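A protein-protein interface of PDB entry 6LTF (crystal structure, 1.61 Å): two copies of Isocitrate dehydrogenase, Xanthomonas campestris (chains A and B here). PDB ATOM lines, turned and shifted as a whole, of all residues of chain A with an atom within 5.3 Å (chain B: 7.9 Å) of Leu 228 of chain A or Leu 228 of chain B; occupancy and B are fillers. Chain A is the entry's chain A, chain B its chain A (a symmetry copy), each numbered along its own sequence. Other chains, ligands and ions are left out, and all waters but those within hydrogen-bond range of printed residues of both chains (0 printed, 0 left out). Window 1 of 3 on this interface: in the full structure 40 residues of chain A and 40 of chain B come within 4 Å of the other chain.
Of the printed residues of chain B, Leu 228 of chain A touches Leu 228 (3.8 Å). Leu 228 of chain B touches one residue of chain A. Of the printed residues of chain B, Tyr 125 of chain A touches Lys 174 and Ile 178. Of the printed residues of chain A, Asp 207 of chain B touches Asp 231. Printed residues of chain A within 4 Å of Val 206 of chain B: Ile 232 (3.8 Å). Of the printed residues of chain B, Asp 231 of chain A touches Lys 174 (2.6 Å) and Asp 207 (3.2 Å). Ile 233 of chain B touches none of the printed residues of chain A. Glu 119 of chain B touches none of the printed residues of chain A. The nearest residue of chain B that does not touch Leu 228 of chain A is Phe 229 of chain B (4.1 Å). The nearest residue of chain A that does not touch Leu 228 of chain B is Phe 229 of chain A (4.1 Å).
NZ of Lys 174 of chain B is in salt-bridge range of OD2 of Asp 231 of chain A, at 2.6 Å. The side-chain carboxylate (OD2) of Asp 207 of chain B lies close to the side-chain carboxylate (OD1) of Asp 231 of chain A (3.2 Å).
Along chain B the printed residues that touch a printed residue of chain A span positions 124 to 232. Printed residues of chain A that touch a printed residue of chain B: Ala 124, Tyr 125, Ile 178, Leu 228, Asp 231 and Ile 232. Among the printed residues, Asp or Glu carboxylates within 4 Å of a Lys or Arg side-chain nitrogen of the other chain: Asp 231 of chain A with Lys 174 of chain B.
Among the printed residues, pairs that only touch across the chains: Ala 124 of chain A with Ile 178 of chain B (3.6 Å), Tyr 125 of chain A with Lys 174 of chain B (3.4 Å), Tyr 125 of chain A with Ile 178 of chain B (3.7 Å), Ile 178 of chain A with Ala 124 of chain B (3.6 Å), Ile 178 of chain A with Tyr 125 of chain B (3.7 Å), Leu 228 of chain A with Leu 228 of chain B (3.8 Å), Ile 232 of chain A with Val 206 of chain B (3.8 Å) and Ile 232 of chain A with Ile 232 of chain B (3.9 Å).
Ala 124 of chain A touches Ile 178 of chain B, and with the chains exchanged Ile 178 of chain A touches Ala 124 of chain B. Tyr 125 of chain A touches Ile 178 of chain B, and with the chains exchanged Ile 178 of chain A touches Tyr 125 of chain B. Leu 228 of chain B touches its own counterpart, Leu 228 of chain A. Ile 232 of chain A touches its own counterpart, Ile 232 of chain B.
The side-chain carboxylate of Asp 231 of chain A lies within hydrogen-bond range of the side-chain hydroxyl of Tyr 125 of chain A (2.7 Å). The guanidinium group of Arg 118 of chain A lies within salt-bridge range of the side-chain carboxylate of Asp 231 of chain A, at 3.7 Å. OD2 of Asp 231 of chain B lies within hydrogen-bond range of OH of Tyr 125 of chain B (2.7 Å). The side-chain carboxylate (OD2) of Asp 207 of chain B is in salt-bridge range of the side-chain amino group (NZ) of Lys 174 of chain B (3.1 Å).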
ATOM      1  N   ARG A 118     -22.665  13.787  -2.276  1.00  0.00           N
ATOM      2  CA  ARG A 118     -22.054  12.498  -2.579  1.00  0.00           C
ATOM      3  C   ARG A 118     -23.005  11.674  -3.437  1.00  0.00           C
ATOM      4  O   ARG A 118     -24.152  11.434  -3.026  1.00  0.00           O
ATOM      5  CB  ARG A 118     -21.766  11.779  -1.263  1.00  0.00           C
ATOM      6  CG  ARG A 118     -21.403  10.313  -1.385  1.00  0.00           C
ATOM      7  CD  ARG A 118     -21.431   9.688   0.022  1.00  0.00           C
ATOM      8  NE  ARG A 118     -21.170   8.247  -0.050  1.00  0.00           N
ATOM      9  CZ  ARG A 118     -21.342   7.398   0.955  1.00  0.00           C
ATOM     10  NH1 ARG A 118     -21.770   7.821   2.152  1.00  0.00           N
ATOM     11  NH2 ARG A 118     -21.073   6.112   0.762  1.00  0.00           N
ATOM     12  N   ALA A 124     -17.741   3.123  -6.691  1.00  0.00           N
ATOM     13  CA  ALA A 124     -16.941   1.973  -6.260  1.00  0.00           C
ATOM     14  C   ALA A 124     -17.585   1.135  -5.159  1.00  0.00           C
ATOM     15  O   ALA A 124     -16.946   0.185  -4.684  1.00  0.00           O
ATOM     16  CB  ALA A 124     -15.564   2.463  -5.797  1.00  0.00           C
ATOM     17  N   TYR A 125     -18.812   1.446  -4.738  1.00  0.00           N
ATOM     18  CA  TYR A 125     -19.431   0.804  -3.584  1.00  0.00           C
ATOM     19  C   TYR A 125     -20.556  -0.160  -3.972  1.00  0.00           C
ATOM     20  O   TYR A 125     -21.408  -0.493  -3.141  1.00  0.00           O
ATOM     21  CB  TYR A 125     -19.951   1.864  -2.609  1.00  0.00           C
ATOM     22  CG  TYR A 125     -18.931   2.450  -1.639  1.00  0.00           C
ATOM     23  CD1 TYR A 125     -17.588   2.067  -1.656  1.00  0.00           C
ATOM     24  CD2 TYR A 125     -19.330   3.397  -0.692  1.00  0.00           C
ATOM     25  CE1 TYR A 125     -16.664   2.614  -0.739  1.00  0.00           C
ATOM     26  CE2 TYR A 125     -18.433   3.934   0.217  1.00  0.00           C
ATOM     27  CZ  TYR A 125     -17.108   3.563   0.188  1.00  0.00           C
ATOM     28  OH  TYR A 125     -16.236   4.123   1.114  1.00  0.00           O
ATOM     29  N   ILE A 178      -7.528   7.227 -12.660  1.00  0.00           N
ATOM     30  CA  ILE A 178      -8.695   6.395 -13.001  1.00  0.00           C
ATOM     31  C   ILE A 178      -9.414   7.143 -14.117  1.00  0.00           C
ATOM     32  O   ILE A 178     -10.388   7.868 -13.910  1.00  0.00           O
ATOM     33  CB  ILE A 178      -9.599   6.109 -11.786  1.00  0.00           C
ATOM     34  CG1 ILE A 178      -8.774   5.719 -10.547  1.00  0.00           C
ATOM     35  CG2 ILE A 178     -10.585   4.995 -12.115  1.00  0.00           C
ATOM     36  CD1 ILE A 178      -9.642   5.393  -9.347  1.00  0.00           C
ATOM     37  N   THR A 226     -18.056  11.505  -6.392  1.00  0.00           N
ATOM     38  CA  THR A 226     -18.511  10.133  -6.550  1.00  0.00           C
ATOM     39  C   THR A 226     -18.610   9.447  -5.178  1.00  0.00           C
ATOM     40  O   THR A 226     -18.276  10.019  -4.135  1.00  0.00           O
ATOM     41  CB  THR A 226     -17.577   9.389  -7.513  1.00  0.00           C
ATOM     42  OG1 THR A 226     -16.213   9.710  -7.199  1.00  0.00           O
ATOM     43  CG2 THR A 226     -17.870   9.780  -8.992  1.00  0.00           C
ATOM     44  N   ASN A 227     -19.087   8.198  -5.188  1.00  0.00           N
ATOM     45  CA  ASN A 227     -19.618   7.567  -3.979  1.00  0.00           C
ATOM     46  C   ASN A 227     -18.553   7.406  -2.884  1.00  0.00           C
ATOM     47  O   ASN A 227     -18.697   7.917  -1.753  1.00  0.00           O
ATOM     48  CB  ASN A 227     -20.250   6.221  -4.385  1.00  0.00           C
ATOM     49  CG  ASN A 227     -21.253   5.685  -3.350  1.00  0.00           C
ATOM     50  OD1 ASN A 227     -21.291   6.135  -2.191  1.00  0.00           O
ATOM     51  ND2 ASN A 227     -22.076   4.720  -3.772  1.00  0.00           N
ATOM     52  N   LEU A 228     -17.483   6.676  -3.194  1.00  0.00           N
ATOM     53  CA  LEU A 228     -16.435   6.417  -2.207  1.00  0.00           C
ATOM     54  C   LEU A 228     -15.758   7.721  -1.755  1.00  0.00           C
ATOM     55  O   LEU A 228     -15.572   7.960  -0.545  1.00  0.00           O
ATOM     56  CB  LEU A 228     -15.430   5.423  -2.825  1.00  0.00           C
ATOM     57  CG  LEU A 228     -14.144   4.964  -2.112  1.00  0.00           C
ATOM     58  CD1 LEU A 228     -13.555   3.711  -2.802  1.00  0.00           C
ATOM     59  CD2 LEU A 228     -13.082   6.062  -2.056  1.00  0.00           C
ATOM     60  N   PHE A 229     -15.393   8.577  -2.720  1.00  0.00           N
ATOM     61  CA  PHE A 229     -14.761   9.856  -2.386  1.00  0.00           C
ATOM     62  C   PHE A 229     -15.662  10.683  -1.471  1.00  0.00           C
ATOM     63  O   PHE A 229     -15.171  11.347  -0.548  1.00  0.00           O
ATOM     64  CB  PHE A 229     -14.429  10.668  -3.654  1.00  0.00           C
ATOM     65  CG  PHE A 229     -13.317  10.100  -4.509  1.00  0.00           C
ATOM     66  CD1 PHE A 229     -12.450   9.120  -4.040  1.00  0.00           C
ATOM     67  CD2 PHE A 229     -13.131  10.601  -5.801  1.00  0.00           C
ATOM     68  CE1 PHE A 229     -11.418   8.632  -4.871  1.00  0.00           C
ATOM     69  CE2 PHE A 229     -12.123  10.112  -6.635  1.00  0.00           C
ATOM     70  CZ  PHE A 229     -11.263   9.128  -6.158  1.00  0.00           C
ATOM     71  N   GLY A 230     -16.983  10.666  -1.720  1.00  0.00           N
ATOM     72  CA  GLY A 230     -17.904  11.452  -0.900  1.00  0.00           C
ATOM     73  C   GLY A 230     -18.050  10.910   0.509  1.00  0.00           C
ATOM     74  O   GLY A 230     -18.147  11.681   1.472  1.00  0.00           O
ATOM     75  N   ASP A 231     -18.086   9.579   0.651  1.00  0.00           N
ATOM     76  CA  ASP A 231     -18.023   8.955   1.972  1.00  0.00           C
ATOM     77  C   ASP A 231     -16.863   9.527   2.795  1.00  0.00           C
ATOM     78  O   ASP A 231     -17.039  10.078   3.906  1.00  0.00           O
ATOM     79  CB  ASP A 231     -17.866   7.447   1.768  1.00  0.00           C
ATOM     80  CG  ASP A 231     -17.954   6.666   3.050  1.00  0.00           C
ATOM     81  OD1 ASP A 231     -18.667   7.117   3.976  1.00  0.00           O
ATOM     82  OD2 ASP A 231     -17.320   5.582   3.113  1.00  0.00           O
ATOM     83  N   ILE A 232     -15.661   9.437   2.218  1.00  0.00           N
ATOM     84  CA  ILE A 232     -14.455   9.895   2.907  1.00  0.00           C
ATOM     85  C   ILE A 232     -14.532  11.383   3.245  1.00  0.00           C
ATOM     86  O   ILE A 232     -14.294  11.789   4.393  1.00  0.00           O
ATOM     87  CB  ILE A 232     -13.223   9.568   2.056  1.00  0.00           C
ATOM     88  CG1 ILE A 232     -13.012   8.043   2.060  1.00  0.00           C
ATOM     89  CG2 ILE A 232     -11.989  10.338   2.551  1.00  0.00           C
ATOM     90  CD1 ILE A 232     -11.818   7.614   1.208  1.00  0.00           C
ATOM     91  N   ILE A 233     -14.854  12.217   2.249  1.00  0.00           N
ATOM     92  CA  ILE A 233     -14.788  13.659   2.461  1.00  0.00           C
ATOM     93  C   ILE A 233     -15.819  14.115   3.498  1.00  0.00           C
ATOM     94  O   ILE A 233     -15.530  15.003   4.313  1.00  0.00           O
ATOM     95  CB  ILE A 233     -14.932  14.401   1.120  1.00  0.00           C
ATOM     96  CG1 ILE A 233     -13.634  14.220   0.334  1.00  0.00           C
ATOM     97  CG2 ILE A 233     -15.236  15.912   1.348  1.00  0.00           C
ATOM     98  CD1 ILE A 233     -13.690  14.659  -1.131  1.00  0.00           C
ATOM     99  N   ARG B 118       1.518   3.059   2.186  1.00  0.00           N
ATOM    100  CA  ARG B 118       0.524   2.917   1.130  1.00  0.00           C
ATOM    101  C   ARG B 118       0.960   1.824   0.164  1.00  0.00           C
ATOM    102  O   ARG B 118       2.064   1.905  -0.398  1.00  0.00           O
ATOM    103  CB  ARG B 118       0.400   4.253   0.400  1.00  0.00           C
ATOM    104  CG  ARG B 118      -0.365   4.217  -0.907  1.00  0.00           C
ATOM    105  CD  ARG B 118      -0.146   5.556  -1.635  1.00  0.00           C
ATOM    106  NE  ARG B 118      -0.797   5.540  -2.948  1.00  0.00           N
ATOM    107  CZ  ARG B 118      -0.609   6.450  -3.895  1.00  0.00           C
ATOM    108  NH1 ARG B 118       0.212   7.491  -3.700  1.00  0.00           N
ATOM    109  NH2 ARG B 118      -1.257   6.322  -5.047  1.00  0.00           N
ATOM    110  N   GLU B 119       0.106   0.800  -0.021  1.00  0.00           N
ATOM    111  CA  GLU B 119       0.362  -0.217  -1.041  1.00  0.00           C
ATOM    112  C   GLU B 119       0.329   0.442  -2.420  1.00  0.00           C
ATOM    113  O   GLU B 119      -0.618   1.161  -2.727  1.00  0.00           O
ATOM    114  CB  GLU B 119      -0.693  -1.326  -0.957  1.00  0.00           C
ATOM    115  CG  GLU B 119      -0.267  -2.629  -1.645  1.00  0.00           C
ATOM    116  CD  GLU B 119      -0.263  -2.549  -3.160  1.00  0.00           C
ATOM    117  OE1 GLU B 119      -1.154  -1.897  -3.758  1.00  0.00           O
ATOM    118  OE2 GLU B 119       0.679  -3.107  -3.754  1.00  0.00           O
ATOM    119  N   ASN B 120       1.342   0.184  -3.268  1.00  0.00           N
ATOM    120  CA  ASN B 120       1.524   0.997  -4.474  1.00  0.00           C
ATOM    121  C   ASN B 120       1.571   0.195  -5.783  1.00  0.00           C
ATOM    122  O   ASN B 120       1.925   0.767  -6.826  1.00  0.00           O
ATOM    123  CB  ASN B 120       2.792   1.860  -4.321  1.00  0.00           C
ATOM    124  CG  ASN B 120       2.655   3.275  -4.960  1.00  0.00           C
ATOM    125  OD1 ASN B 120       1.562   3.826  -5.084  1.00  0.00           O
ATOM    126  ND2 ASN B 120       3.771   3.848  -5.325  1.00  0.00           N
ATOM    127  N   GLU B 122      -1.177  -2.463  -6.582  1.00  0.00           N
ATOM    128  CA  GLU B 122      -2.486  -2.995  -6.977  1.00  0.00           C
ATOM    129  C   GLU B 122      -3.604  -2.102  -6.432  1.00  0.00           C
ATOM    130  O   GLU B 122      -3.465  -0.875  -6.446  1.00  0.00           O
ATOM    131  CB  GLU B 122      -2.625  -4.468  -6.534  1.00  0.00           C
ATOM    132  CG  GLU B 122      -2.348  -4.735  -5.045  1.00  0.00           C
ATOM    133  CD  GLU B 122      -2.396  -6.217  -4.661  1.00  0.00           C
ATOM    134  OE1 GLU B 122      -1.986  -7.092  -5.485  1.00  0.00           O
ATOM    135  OE2 GLU B 122      -2.828  -6.509  -3.519  1.00  0.00           O
ATOM    136  N   GLY B 123      -4.725  -2.679  -5.986  1.00  0.00           N
ATOM    137  CA  GLY B 123      -5.805  -1.824  -5.503  1.00  0.00           C
ATOM    138  C   GLY B 123      -6.568  -1.194  -6.660  1.00  0.00           C
ATOM    139  O   GLY B 123      -6.682  -1.760  -7.750  1.00  0.00           O
ATOM    140  N   ALA B 124      -7.081   0.018  -6.431  1.00  0.00           N
ATOM    141  CA  ALA B 124      -8.024   0.636  -7.368  1.00  0.00           C
ATOM    142  C   ALA B 124      -7.370   1.511  -8.434  1.00  0.00           C
ATOM    143  O   ALA B 124      -8.097   2.129  -9.224  1.00  0.00           O
ATOM    144  CB  ALA B 124      -9.048   1.461  -6.581  1.00  0.00           C
ATOM    145  N   TYR B 125      -6.039   1.587  -8.487  1.00  0.00           N
ATOM    146  CA  TYR B 125      -5.341   2.522  -9.363  1.00  0.00           C
ATOM    147  C   TYR B 125      -4.660   1.831 -10.548  1.00  0.00           C
ATOM    148  O   TYR B 125      -3.746   2.396 -11.159  1.00  0.00           O
ATOM    149  CB  TYR B 125      -4.320   3.331  -8.559  1.00  0.00           C
ATOM    150  CG  TYR B 125      -4.857   4.549  -7.814  1.00  0.00           C
ATOM    151  CD1 TYR B 125      -6.210   4.893  -7.835  1.00  0.00           C
ATOM    152  CD2 TYR B 125      -3.985   5.364  -7.087  1.00  0.00           C
ATOM    153  CE1 TYR B 125      -6.682   6.032  -7.148  1.00  0.00           C
ATOM    154  CE2 TYR B 125      -4.436   6.488  -6.415  1.00  0.00           C
ATOM    155  CZ  TYR B 125      -5.773   6.815  -6.428  1.00  0.00           C
ATOM    156  OH  TYR B 125      -6.191   7.950  -5.742  1.00  0.00           O
ATOM    157  N   GLY B 142     -11.667  -1.145 -12.334  1.00  0.00           N
ATOM    158  CA  GLY B 142     -11.567  -2.301 -11.476  1.00  0.00           C
ATOM    159  C   GLY B 142     -10.621  -2.052 -10.317  1.00  0.00           C
ATOM    160  O   GLY B 142      -9.895  -1.054 -10.266  1.00  0.00           O
ATOM    161  N   ALA B 143     -10.644  -2.989  -9.384  1.00  0.00           N
ATOM    162  CA  ALA B 143      -9.640  -3.056  -8.338  1.00  0.00           C
ATOM    163  C   ALA B 143      -9.279  -4.515  -8.140  1.00  0.00           C
ATOM    164  O   ALA B 143     -10.135  -5.397  -8.265  1.00  0.00           O
ATOM    165  CB  ALA B 143     -10.131  -2.445  -7.018  1.00  0.00           C
ATOM    166  N   LYS B 174     -12.318  -0.586   4.125  1.00  0.00           N
ATOM    167  CA  LYS B 174     -13.768  -0.435   3.985  1.00  0.00           C
ATOM    168  C   LYS B 174     -14.401  -1.807   3.751  1.00  0.00           C
ATOM    169  O   LYS B 174     -15.194  -2.020   2.830  1.00  0.00           O
ATOM    170  CB  LYS B 174     -14.118   0.555   2.860  1.00  0.00           C
ATOM    171  CG  LYS B 174     -15.581   1.000   2.810  1.00  0.00           C
ATOM    172  CD  LYS B 174     -15.892   2.117   3.819  1.00  0.00           C
ATOM    173  CE  LYS B 174     -17.371   2.443   3.852  1.00  0.00           C
ATOM    174  NZ  LYS B 174     -17.666   3.597   4.754  1.00  0.00           N
ATOM    175  N   ILE B 178     -16.978  -2.906   0.659  1.00  0.00           N
ATOM    176  CA  ILE B 178     -16.209  -3.561  -0.414  1.00  0.00           C
ATOM    177  C   ILE B 178     -15.628  -4.821   0.215  1.00  0.00           C
ATOM    178  O   ILE B 178     -14.474  -4.878   0.645  1.00  0.00           O
ATOM    179  CB  ILE B 178     -15.136  -2.640  -1.025  1.00  0.00           C
ATOM    180  CG1 ILE B 178     -15.687  -1.229  -1.293  1.00  0.00           C
ATOM    181  CG2 ILE B 178     -14.608  -3.238  -2.324  1.00  0.00           C
ATOM    182  CD1 ILE B 178     -14.661  -0.313  -1.932  1.00  0.00           C
ATOM    183  N   VAL B 206     -12.144   3.606   6.868  1.00  0.00           N
ATOM    184  CA  VAL B 206     -11.420   4.736   6.270  1.00  0.00           C
ATOM    185  C   VAL B 206     -12.122   6.072   6.558  1.00  0.00           C
ATOM    186  O   VAL B 206     -11.459   7.100   6.757  1.00  0.00           O
ATOM    187  CB  VAL B 206     -11.214   4.506   4.757  1.00  0.00           C
ATOM    188  CG1 VAL B 206     -12.566   4.315   4.030  1.00  0.00           C
ATOM    189  CG2 VAL B 206     -10.373   5.633   4.121  1.00  0.00           C
ATOM    190  N   ASP B 207     -13.457   6.098   6.558  1.00  0.00           N
ATOM    191  CA  ASP B 207     -14.116   7.383   6.807  1.00  0.00           C
ATOM    192  C   ASP B 207     -13.877   7.851   8.247  1.00  0.00           C
ATOM    193  O   ASP B 207     -13.515   9.020   8.497  1.00  0.00           O
ATOM    194  CB  ASP B 207     -15.610   7.312   6.452  1.00  0.00           C
ATOM    195  CG  ASP B 207     -16.354   6.108   7.024  1.00  0.00           C
ATOM    196  OD1 ASP B 207     -15.794   5.269   7.757  1.00  0.00           O
ATOM    197  OD2 ASP B 207     -17.576   6.026   6.730  1.00  0.00           O
ATOM    198  N   THR B 225      -2.404   0.784   4.516  1.00  0.00           N
ATOM    199  CA  THR B 225      -3.649   0.710   3.754  1.00  0.00           C
ATOM    200  C   THR B 225      -3.352   0.479   2.276  1.00  0.00           C
ATOM    201  O   THR B 225      -2.196   0.408   1.839  1.00  0.00           O
ATOM    202  CB  THR B 225      -4.505   1.975   3.965  1.00  0.00           C
ATOM    203  OG1 THR B 225      -5.864   1.742   3.538  1.00  0.00           O
ATOM    204  CG2 THR B 225      -3.907   3.153   3.231  1.00  0.00           C
ATOM    205  N   THR B 226      -4.437   0.320   1.528  1.00  0.00           N
ATOM    206  CA  THR B 226      -4.428   0.029   0.104  1.00  0.00           C
ATOM    207  C   THR B 226      -4.168   1.314  -0.698  1.00  0.00           C
ATOM    208  O   THR B 226      -4.054   2.415  -0.150  1.00  0.00           O
ATOM    209  CB  THR B 226      -5.745  -0.654  -0.289  1.00  0.00           C
ATOM    210  OG1 THR B 226      -6.841   0.022   0.345  1.00  0.00           O
ATOM    211  CG2 THR B 226      -5.749  -2.152   0.136  1.00  0.00           C
ATOM    212  N   ASN B 227      -4.068   1.160  -2.022  1.00  0.00           N
ATOM    213  CA  ASN B 227      -3.435   2.172  -2.869  1.00  0.00           C
ATOM    214  C   ASN B 227      -4.183   3.513  -2.842  1.00  0.00           C
ATOM    215  O   ASN B 227      -3.619   4.568  -2.483  1.00  0.00           O
ATOM    216  CB  ASN B 227      -3.319   1.593  -4.293  1.00  0.00           C
ATOM    217  CG  ASN B 227      -2.267   2.311  -5.155  1.00  0.00           C
ATOM    218  OD1 ASN B 227      -1.811   3.421  -4.830  1.00  0.00           O
ATOM    219  ND2 ASN B 227      -1.874   1.670  -6.260  1.00  0.00           N
ATOM    220  N   LEU B 228      -5.453   3.495  -3.242  1.00  0.00           N
ATOM    221  CA  LEU B 228      -6.241   4.727  -3.305  1.00  0.00           C
ATOM    222  C   LEU B 228      -6.399   5.361  -1.913  1.00  0.00           C
ATOM    223  O   LEU B 228      -6.193   6.579  -1.737  1.00  0.00           O
ATOM    224  CB  LEU B 228      -7.603   4.393  -3.949  1.00  0.00           C
ATOM    225  CG  LEU B 228      -8.735   5.422  -4.119  1.00  0.00           C
ATOM    226  CD1 LEU B 228      -9.800   4.903  -5.115  1.00  0.00           C
ATOM    227  CD2 LEU B 228      -9.407   5.778  -2.793  1.00  0.00           C
ATOM    228  N   PHE B 229      -6.754   4.542  -0.913  1.00  0.00           N
ATOM    229  CA  PHE B 229      -6.907   5.051   0.452  1.00  0.00           C
ATOM    230  C   PHE B 229      -5.610   5.696   0.938  1.00  0.00           C
ATOM    231  O   PHE B 229      -5.647   6.726   1.626  1.00  0.00           O
ATOM    232  CB  PHE B 229      -7.321   3.930   1.427  1.00  0.00           C
ATOM    233  CG  PHE B 229      -8.727   3.402   1.240  1.00  0.00           C
ATOM    234  CD1 PHE B 229      -9.676   4.077   0.480  1.00  0.00           C
ATOM    235  CD2 PHE B 229      -9.097   2.215   1.879  1.00  0.00           C
ATOM    236  CE1 PHE B 229     -10.979   3.552   0.348  1.00  0.00           C
ATOM    237  CE2 PHE B 229     -10.379   1.680   1.740  1.00  0.00           C
ATOM    238  CZ  PHE B 229     -11.321   2.361   0.975  1.00  0.00           C
ATOM    239  N   GLY B 230      -4.454   5.098   0.602  1.00  0.00           N
ATOM    240  CA  GLY B 230      -3.176   5.646   1.052  1.00  0.00           C
ATOM    241  C   GLY B 230      -2.823   6.957   0.373  1.00  0.00           C
ATOM    242  O   GLY B 230      -2.276   7.866   1.008  1.00  0.00           O
ATOM    243  N   ASP B 231      -3.115   7.068  -0.930  1.00  0.00           N
ATOM    244  CA  ASP B 231      -3.002   8.348  -1.625  1.00  0.00           C
ATOM    245  C   ASP B 231      -3.710   9.462  -0.845  1.00  0.00           C
ATOM    246  O   ASP B 231      -3.110  10.491  -0.455  1.00  0.00           O
ATOM    247  CB  ASP B 231      -3.609   8.177  -3.019  1.00  0.00           C
ATOM    248  CG  ASP B 231      -3.408   9.377  -3.903  1.00  0.00           C
ATOM    249  OD1 ASP B 231      -2.386  10.080  -3.731  1.00  0.00           O
ATOM    250  OD2 ASP B 231      -4.274   9.597  -4.787  1.00  0.00           O
ATOM    251  N   ILE B 232      -4.997   9.232  -0.573  1.00  0.00           N
ATOM    252  CA  ILE B 232      -5.813  10.228   0.121  1.00  0.00           C
ATOM    253  C   ILE B 232      -5.251  10.550   1.504  1.00  0.00           C
ATOM    254  O   ILE B 232      -5.065  11.725   1.859  1.00  0.00           O
ATOM    255  CB  ILE B 232      -7.264   9.739   0.196  1.00  0.00           C
ATOM    256  CG1 ILE B 232      -7.873   9.782  -1.217  1.00  0.00           C
ATOM    257  CG2 ILE B 232      -8.072  10.559   1.213  1.00  0.00           C
ATOM    258  CD1 ILE B 232      -9.316   9.281  -1.250  1.00  0.00           C
ATOM    259  N   ILE B 233      -4.983   9.514   2.308  1.00  0.00           N
ATOM    260  CA  ILE B 233      -4.599   9.753   3.695  1.00  0.00           C
ATOM    261  C   ILE B 233      -3.251  10.477   3.780  1.00  0.00           C
ATOM    262  O   ILE B 233      -3.068  11.350   4.640  1.00  0.00           O
ATOM    263  CB  ILE B 233      -4.609   8.433   4.485  1.00  0.00           C
ATOM    264  CG1 ILE B 233      -6.065   8.026   4.713  1.00  0.00           C
ATOM    265  CG2 ILE B 233      -3.859   8.587   5.842  1.00  0.00           C
ATOM    266  CD1 ILE B 233      -6.272   6.606   5.245  1.00  0.00           C
ATOM    267  N   SER B 234      -2.295  10.146   2.908  1.00  0.00           N
ATOM    268  CA  SER B 234      -0.992  10.797   3.013  1.00  0.00           C
ATOM    269  C   SER B 234      -1.096  12.289   2.708  1.00  0.00           C
ATOM    270  O   SER B 234      -0.437  13.107   3.364  1.00  0.00           O
ATOM    271  CB  SER B 234       0.037  10.110   2.109  1.00  0.00           C
ATOM    272  OG  SER B 234      -0.307  10.173   0.732  1.00  0.00           O
